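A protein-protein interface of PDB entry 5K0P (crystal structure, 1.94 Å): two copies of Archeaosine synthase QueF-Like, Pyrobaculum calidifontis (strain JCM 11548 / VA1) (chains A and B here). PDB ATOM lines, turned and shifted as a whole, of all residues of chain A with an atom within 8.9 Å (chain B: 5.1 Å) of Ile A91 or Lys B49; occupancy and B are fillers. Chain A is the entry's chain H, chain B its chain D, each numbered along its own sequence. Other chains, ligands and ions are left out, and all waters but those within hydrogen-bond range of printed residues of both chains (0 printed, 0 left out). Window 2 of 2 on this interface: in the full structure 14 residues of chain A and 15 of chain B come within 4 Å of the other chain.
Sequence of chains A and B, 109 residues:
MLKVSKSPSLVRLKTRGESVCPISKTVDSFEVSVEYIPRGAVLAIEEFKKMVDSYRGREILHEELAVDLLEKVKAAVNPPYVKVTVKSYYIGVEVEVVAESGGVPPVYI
Among the printed residues, merely in contact across the chains: Tyr A90 with Ile B45 (3.7 Å), Ile A91 with Ile B45 (3.95 Å), Ile A91 with Glu B46 (3.8 Å), Ile A91 with Lys B49 (3.3 Å), Val A93 with Ile B45 (3.8 Å) and Val A93 with Phe B48 (3.996 Å).
Of the 11 printed residues of chain A, 3 touch a printed residue of chain B. Printed residues of chain A that touch a printed residue of chain B: Tyr A90, Ile A91 and Val A93. Hydrophobic or aromatic side chains of chain B that line the printed part of chain A: Ile B45 and Phe B48. Among the printed residues, 7 pairs touch across the chains.
The side-chain carboxylate of Asp B53 is in salt-bridge range of the side-chain amino group of Lys B49.
No position is printed for both chains. Of the 7 pairs that touch across the chains among the printed residues, none has its exchanged pair printed and touching as well.
Of the printed residues of chain B, Ile A91 touches Ile B45, Glu B46 and Lys B49. Of chain A, only Ile A91 comes within 4 Å of Lys B49. Of the printed residues of chain A, Ile B45 touches Tyr A90, Ile A91 and Val A93. Of the printed residues of chain B, Tyr A90 touches Ile B45 (3.7 Å) and Glu B46 (2.6 Å). Cys A21 touches none of the printed residues of chain B. Met B51 touches none of the printed residues of chain A. The nearest printed residue of chain A that does not touch Glu B46 is Ile A23 (4.8 Å).
The side-chain carboxylate (OE2) of Glu B46 lies within hydrogen-bond range of the side-chain hydroxyl (OH) of Tyr A90 (2.6 Å).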
ATOM      1  N   CYS A  21      11.025 -32.220 -24.289  1.00  0.00           N
ATOM      2  CA  CYS A  21      10.567 -31.550 -23.097  1.00  0.00           C
ATOM      3  C   CYS A  21      10.042 -32.584 -22.127  1.00  0.00           C
ATOM      4  O   CYS A  21       9.135 -33.334 -22.484  1.00  0.00           O
ATOM      5  CB  CYS A  21       9.452 -30.609 -23.472  1.00  0.00           C
ATOM      6  SG  CYS A  21       8.619 -30.056 -22.001  1.00  0.00           S
ATOM      7  N   ILE A  23       8.188 -32.524 -19.530  1.00  0.00           N
ATOM      8  CA  ILE A  23       6.795 -32.399 -19.116  1.00  0.00           C
ATOM      9  C   ILE A  23       5.803 -32.796 -20.215  1.00  0.00           C
ATOM     10  O   ILE A  23       4.974 -33.617 -19.945  1.00  0.00           O
ATOM     11  CB  ILE A  23       6.421 -31.057 -18.403  1.00  0.00           C
ATOM     12  CG1 ILE A  23       4.848 -30.857 -18.341  1.00  0.00           C
ATOM     13  CG2 ILE A  23       7.125 -29.815 -18.928  1.00  0.00           C
ATOM     14  CD1 ILE A  23       4.136 -31.773 -17.327  1.00  0.00           C
ATOM     15  N   ASP A  28      11.812 -30.069 -28.453  1.00  0.00           N
ATOM     16  CA  ASP A  28      12.175 -28.794 -27.887  1.00  0.00           C
ATOM     17  C   ASP A  28      13.494 -28.367 -28.584  1.00  0.00           C
ATOM     18  O   ASP A  28      14.599 -28.845 -28.214  1.00  0.00           O
ATOM     19  CB  ASP A  28      12.418 -29.048 -26.381  1.00  0.00           C
ATOM     20  CG  ASP A  28      12.511 -27.809 -25.577  1.00  0.00           C
ATOM     21  OD1 ASP A  28      12.425 -26.720 -26.205  1.00  0.00           O
ATOM     22  OD2 ASP A  28      12.695 -27.946 -24.308  1.00  0.00           O
ATOM     23  N   SER A  88      16.823 -21.128 -26.109  1.00  0.00           N
ATOM     24  CA  SER A  88      15.623 -21.638 -26.617  1.00  0.00           C
ATOM     25  C   SER A  88      14.431 -20.719 -26.213  1.00  0.00           C
ATOM     26  O   SER A  88      14.584 -19.688 -25.604  1.00  0.00           O
ATOM     27  CB  SER A  88      15.454 -23.085 -26.102  1.00  0.00           C
ATOM     28  OG  SER A  88      15.732 -23.158 -24.720  1.00  0.00           O
ATOM     29  N   TYR A  89      13.232 -21.117 -26.582  1.00  0.00           N
ATOM     30  CA  TYR A  89      12.064 -20.266 -26.463  1.00  0.00           C
ATOM     31  C   TYR A  89      10.930 -21.126 -25.994  1.00  0.00           C
ATOM     32  O   TYR A  89      10.597 -22.159 -26.572  1.00  0.00           O
ATOM     33  CB  TYR A  89      11.835 -19.591 -27.814  1.00  0.00           C
ATOM     34  CG  TYR A  89      10.743 -18.567 -27.871  1.00  0.00           C
ATOM     35  CD1 TYR A  89      10.889 -17.361 -27.180  1.00  0.00           C
ATOM     36  CD2 TYR A  89       9.578 -18.740 -28.710  1.00  0.00           C
ATOM     37  CE1 TYR A  89       9.901 -16.365 -27.231  1.00  0.00           C
ATOM     38  CE2 TYR A  89       8.596 -17.730 -28.802  1.00  0.00           C
ATOM     39  CZ  TYR A  89       8.768 -16.536 -28.051  1.00  0.00           C
ATOM     40  OH  TYR A  89       7.852 -15.462 -28.079  1.00  0.00           O
ATOM     41  N   TYR A  90      10.342 -20.730 -24.898  1.00  0.00           N
ATOM     42  CA  TYR A  90       9.448 -21.602 -24.183  1.00  0.00           C
ATOM     43  C   TYR A  90       8.381 -20.747 -23.500  1.00  0.00           C
ATOM     44  O   TYR A  90       8.743 -19.841 -22.745  1.00  0.00           O
ATOM     45  CB  TYR A  90      10.241 -22.468 -23.161  1.00  0.00           C
ATOM     46  CG  TYR A  90       9.359 -23.414 -22.340  1.00  0.00           C
ATOM     47  CD1 TYR A  90       8.617 -24.472 -22.949  1.00  0.00           C
ATOM     48  CD2 TYR A  90       9.237 -23.244 -20.962  1.00  0.00           C
ATOM     49  CE1 TYR A  90       7.770 -25.313 -22.177  1.00  0.00           C
ATOM     50  CE2 TYR A  90       8.419 -24.060 -20.195  1.00  0.00           C
ATOM     51  CZ  TYR A  90       7.671 -25.089 -20.784  1.00  0.00           C
ATOM     52  OH  TYR A  90       6.874 -25.861 -19.937  1.00  0.00           O
ATOM     53  N   ILE A  91       7.111 -21.068 -23.755  1.00  0.00           N
ATOM     54  CA  ILE A  91       5.959 -20.385 -23.222  1.00  0.00           C
ATOM     55  C   ILE A  91       6.117 -18.893 -23.358  1.00  0.00           C
ATOM     56  O   ILE A  91       5.736 -18.139 -22.484  1.00  0.00           O
ATOM     57  CB  ILE A  91       5.500 -20.854 -21.808  1.00  0.00           C
ATOM     58  CG1 ILE A  91       6.599 -20.658 -20.712  1.00  0.00           C
ATOM     59  CG2 ILE A  91       5.110 -22.328 -21.924  1.00  0.00           C
ATOM     60  CD1 ILE A  91       6.224 -21.101 -19.284  1.00  0.00           C
ATOM     61  N   GLY A  92       6.607 -18.474 -24.503  1.00  0.00           N
ATOM     62  CA  GLY A  92       6.841 -17.010 -24.770  1.00  0.00           C
ATOM     63  C   GLY A  92       8.003 -16.386 -24.006  1.00  0.00           C
ATOM     64  O   GLY A  92       8.084 -15.198 -23.968  1.00  0.00           O
ATOM     65  N   VAL A  93       8.886 -17.186 -23.410  1.00  0.00           N
ATOM     66  CA  VAL A  93      10.114 -16.712 -22.748  1.00  0.00           C
ATOM     67  C   VAL A  93      11.324 -17.098 -23.585  1.00  0.00           C
ATOM     68  O   VAL A  93      11.460 -18.279 -23.941  1.00  0.00           O
ATOM     69  CB  VAL A  93      10.250 -17.279 -21.310  1.00  0.00           C
ATOM     70  CG1 VAL A  93      11.490 -16.719 -20.629  1.00  0.00           C
ATOM     71  CG2 VAL A  93       9.027 -16.926 -20.495  1.00  0.00           C
ATOM     72  N   GLU A  94      12.164 -16.141 -23.946  1.00  0.00           N
ATOM     73  CA  GLU A  94      13.500 -16.419 -24.453  1.00  0.00           C
ATOM     74  C   GLU A  94      14.429 -16.799 -23.298  1.00  0.00           C
ATOM     75  O   GLU A  94      14.607 -16.010 -22.362  1.00  0.00           O
ATOM     76  CB  GLU A  94      14.129 -15.243 -25.167  1.00  0.00           C
ATOM     77  CG  GLU A  94      13.321 -14.783 -26.367  1.00  0.00           C
ATOM     78  CD  GLU A  94      13.874 -13.518 -26.929  1.00  0.00           C
ATOM     79  OE1 GLU A  94      15.119 -13.458 -27.231  1.00  0.00           O
ATOM     80  OE2 GLU A  94      13.049 -12.595 -26.986  1.00  0.00           O
ATOM     81  N   VAL A  95      15.009 -17.985 -23.385  1.00  0.00           N
ATOM     82  CA  VAL A  95      15.832 -18.523 -22.325  1.00  0.00           C
ATOM     83  C   VAL A  95      17.279 -18.715 -22.865  1.00  0.00           C
ATOM     84  O   VAL A  95      17.459 -19.252 -23.957  1.00  0.00           O
ATOM     85  CB  VAL A  95      15.302 -19.884 -21.864  1.00  0.00           C
ATOM     86  CG1 VAL A  95      16.132 -20.349 -20.640  1.00  0.00           C
ATOM     87  CG2 VAL A  95      13.803 -19.848 -21.543  1.00  0.00           C
ATOM     88  N   ALA B  44      12.152 -21.940 -12.115  1.00  0.00           N
ATOM     89  CA  ALA B  44      11.358 -22.548 -13.240  1.00  0.00           C
ATOM     90  C   ALA B  44      10.823 -21.513 -14.214  1.00  0.00           C
ATOM     91  O   ALA B  44      10.302 -20.479 -13.804  1.00  0.00           O
ATOM     92  CB  ALA B  44      10.175 -23.344 -12.658  1.00  0.00           C
ATOM     93  N   ILE B  45      10.872 -21.794 -15.498  1.00  0.00           N
ATOM     94  CA  ILE B  45      10.380 -20.813 -16.502  1.00  0.00           C
ATOM     95  C   ILE B  45       8.886 -20.512 -16.264  1.00  0.00           C
ATOM     96  O   ILE B  45       8.472 -19.379 -16.375  1.00  0.00           O
ATOM     97  CB  ILE B  45      10.528 -21.298 -17.974  1.00  0.00           C
ATOM     98  CG1 ILE B  45      11.932 -21.857 -18.357  1.00  0.00           C
ATOM     99  CG2 ILE B  45      10.115 -20.226 -18.962  1.00  0.00           C
ATOM    100  CD1 ILE B  45      13.075 -21.182 -17.726  1.00  0.00           C
ATOM    101  N   GLU B  46       8.123 -21.572 -16.025  1.00  0.00           N
ATOM    102  CA  GLU B  46       6.736 -21.492 -15.580  1.00  0.00           C
ATOM    103  C   GLU B  46       6.511 -20.430 -14.466  1.00  0.00           C
ATOM    104  O   GLU B  46       5.623 -19.568 -14.571  1.00  0.00           O
ATOM    105  CB  GLU B  46       6.290 -22.875 -15.093  1.00  0.00           C
ATOM    106  CG  GLU B  46       6.280 -23.971 -16.159  1.00  0.00           C
ATOM    107  CD  GLU B  46       7.624 -24.563 -16.510  1.00  0.00           C
ATOM    108  OE1 GLU B  46       8.651 -24.335 -15.877  1.00  0.00           O
ATOM    109  OE2 GLU B  46       7.625 -25.321 -17.460  1.00  0.00           O
ATOM    110  N   GLU B  47       7.338 -20.497 -13.431  1.00  0.00           N
ATOM    111  CA  GLU B  47       7.238 -19.654 -12.308  1.00  0.00           C
ATOM    112  C   GLU B  47       7.641 -18.206 -12.694  1.00  0.00           C
ATOM    113  O   GLU B  47       6.959 -17.246 -12.299  1.00  0.00           O
ATOM    114  CB  GLU B  47       8.065 -20.263 -11.158  1.00  0.00           C
ATOM    115  CG  GLU B  47       7.653 -19.909  -9.727  1.00  0.00           C
ATOM    116  CD  GLU B  47       6.188 -19.619  -9.525  1.00  0.00           C
ATOM    117  OE1 GLU B  47       5.392 -20.574  -9.790  1.00  0.00           O
ATOM    118  OE2 GLU B  47       5.890 -18.441  -9.090  1.00  0.00           O
ATOM    119  N   PHE B  48       8.679 -18.033 -13.487  1.00  0.00           N
ATOM    120  CA  PHE B  48       9.000 -16.695 -14.012  1.00  0.00           C
ATOM    121  C   PHE B  48       7.866 -16.094 -14.812  1.00  0.00           C
ATOM    122  O   PHE B  48       7.544 -14.941 -14.637  1.00  0.00           O
ATOM    123  CB  PHE B  48      10.261 -16.754 -14.905  1.00  0.00           C
ATOM    124  CG  PHE B  48      10.576 -15.464 -15.620  1.00  0.00           C
ATOM    125  CD1 PHE B  48      10.969 -14.381 -14.917  1.00  0.00           C
ATOM    126  CD2 PHE B  48      10.457 -15.354 -16.985  1.00  0.00           C
ATOM    127  CE1 PHE B  48      11.270 -13.189 -15.547  1.00  0.00           C
ATOM    128  CE2 PHE B  48      10.739 -14.174 -17.641  1.00  0.00           C
ATOM    129  CZ  PHE B  48      11.171 -13.102 -16.917  1.00  0.00           C
ATOM    130  N   LYS B  49       7.236 -16.900 -15.658  1.00  0.00           N
ATOM    131  CA  LYS B  49       6.174 -16.369 -16.463  1.00  0.00           C
ATOM    132  C   LYS B  49       4.967 -16.007 -15.581  1.00  0.00           C
ATOM    133  O   LYS B  49       4.337 -14.995 -15.791  1.00  0.00           O
ATOM    134  CB  LYS B  49       5.807 -17.331 -17.570  1.00  0.00           C
ATOM    135  CG  LYS B  49       4.596 -16.883 -18.365  1.00  0.00           C
ATOM    136  CD  LYS B  49       4.299 -17.748 -19.558  1.00  0.00           C
ATOM    137  CE  LYS B  49       2.824 -17.689 -20.006  1.00  0.00           C
ATOM    138  NZ  LYS B  49       2.354 -16.312 -20.278  1.00  0.00           N
ATOM    139  N   LYS B  50       4.692 -16.776 -14.543  1.00  0.00           N
ATOM    140  CA  LYS B  50       3.652 -16.363 -13.577  1.00  0.00           C
ATOM    141  C   LYS B  50       3.988 -15.046 -12.930  1.00  0.00           C
ATOM    142  O   LYS B  50       3.092 -14.200 -12.804  1.00  0.00           O
ATOM    143  CB  LYS B  50       3.295 -17.435 -12.520  1.00  0.00           C
ATOM    144  CG  LYS B  50       2.682 -16.858 -11.207  1.00  0.00           C
ATOM    145  CD  LYS B  50       2.767 -17.673  -9.862  1.00  0.00           C
ATOM    146  CE  LYS B  50       1.764 -18.816  -9.794  1.00  0.00           C
ATOM    147  NZ  LYS B  50       2.143 -19.852 -10.824  1.00  0.00           N
ATOM    148  N   MET B  51       5.242 -14.896 -12.489  1.00  0.00           N
ATOM    149  CA  MET B  51       5.688 -13.639 -11.856  1.00  0.00           C
ATOM    150  C   MET B  51       5.433 -12.462 -12.785  1.00  0.00           C
ATOM    151  O   MET B  51       4.924 -11.427 -12.329  1.00  0.00           O
ATOM    152  CB  MET B  51       7.174 -13.679 -11.498  1.00  0.00           C
ATOM    153  CG  MET B  51       7.545 -14.675 -10.381  1.00  0.00           C
ATOM    154  SD  MET B  51       9.340 -14.544 -10.217  1.00  0.00           S
ATOM    155  CE  MET B  51       9.618 -15.659  -8.837  1.00  0.00           C
ATOM    156  N   VAL B  52       5.768 -12.641 -14.065  1.00  0.00           N
ATOM    157  CA  VAL B  52       5.543 -11.575 -15.053  1.00  0.00           C
ATOM    158  C   VAL B  52       4.033 -11.303 -15.331  1.00  0.00           C
ATOM    159  O   VAL B  52       3.606 -10.139 -15.381  1.00  0.00           O
ATOM    160  CB  VAL B  52       6.355 -11.798 -16.344  1.00  0.00           C
ATOM    161  CG1 VAL B  52       5.982 -10.760 -17.387  1.00  0.00           C
ATOM    162  CG2 VAL B  52       7.847 -11.775 -15.982  1.00  0.00           C
ATOM    163  N   ASP B  53       3.252 -12.367 -15.471  1.00  0.00           N
ATOM    164  CA  ASP B  53       1.857 -12.230 -15.709  1.00  0.00           C
ATOM    165  C   ASP B  53       1.097 -11.674 -14.512  1.00  0.00           C
ATOM    166  O   ASP B  53       0.000 -11.168 -14.701  1.00  0.00           O
ATOM    167  CB  ASP B  53       1.214 -13.558 -16.184  1.00  0.00           C
ATOM    168  CG  ASP B  53       1.641 -13.938 -17.623  1.00  0.00           C
ATOM    169  OD1 ASP B  53       2.118 -13.066 -18.388  1.00  0.00           O
ATOM    170  OD2 ASP B  53       1.498 -15.114 -18.032  1.00  0.00           O
ATOM    171  N   SER B  54       1.668 -11.698 -13.305  1.00  0.00           N
ATOM    172  CA  SER B  54       0.977 -11.168 -12.142  1.00  0.00           C
ATOM    173  C   SER B  54       0.732  -9.656 -12.219  1.00  0.00           C
ATOM    174  O   SER B  54      -0.166  -9.131 -11.499  1.00  0.00           O
ATOM    175  CB  SER B  54       1.757 -11.465 -10.846  1.00  0.00           C
ATOM    176  OG  SER B  54       2.900 -10.596 -10.744  1.00  0.00           O
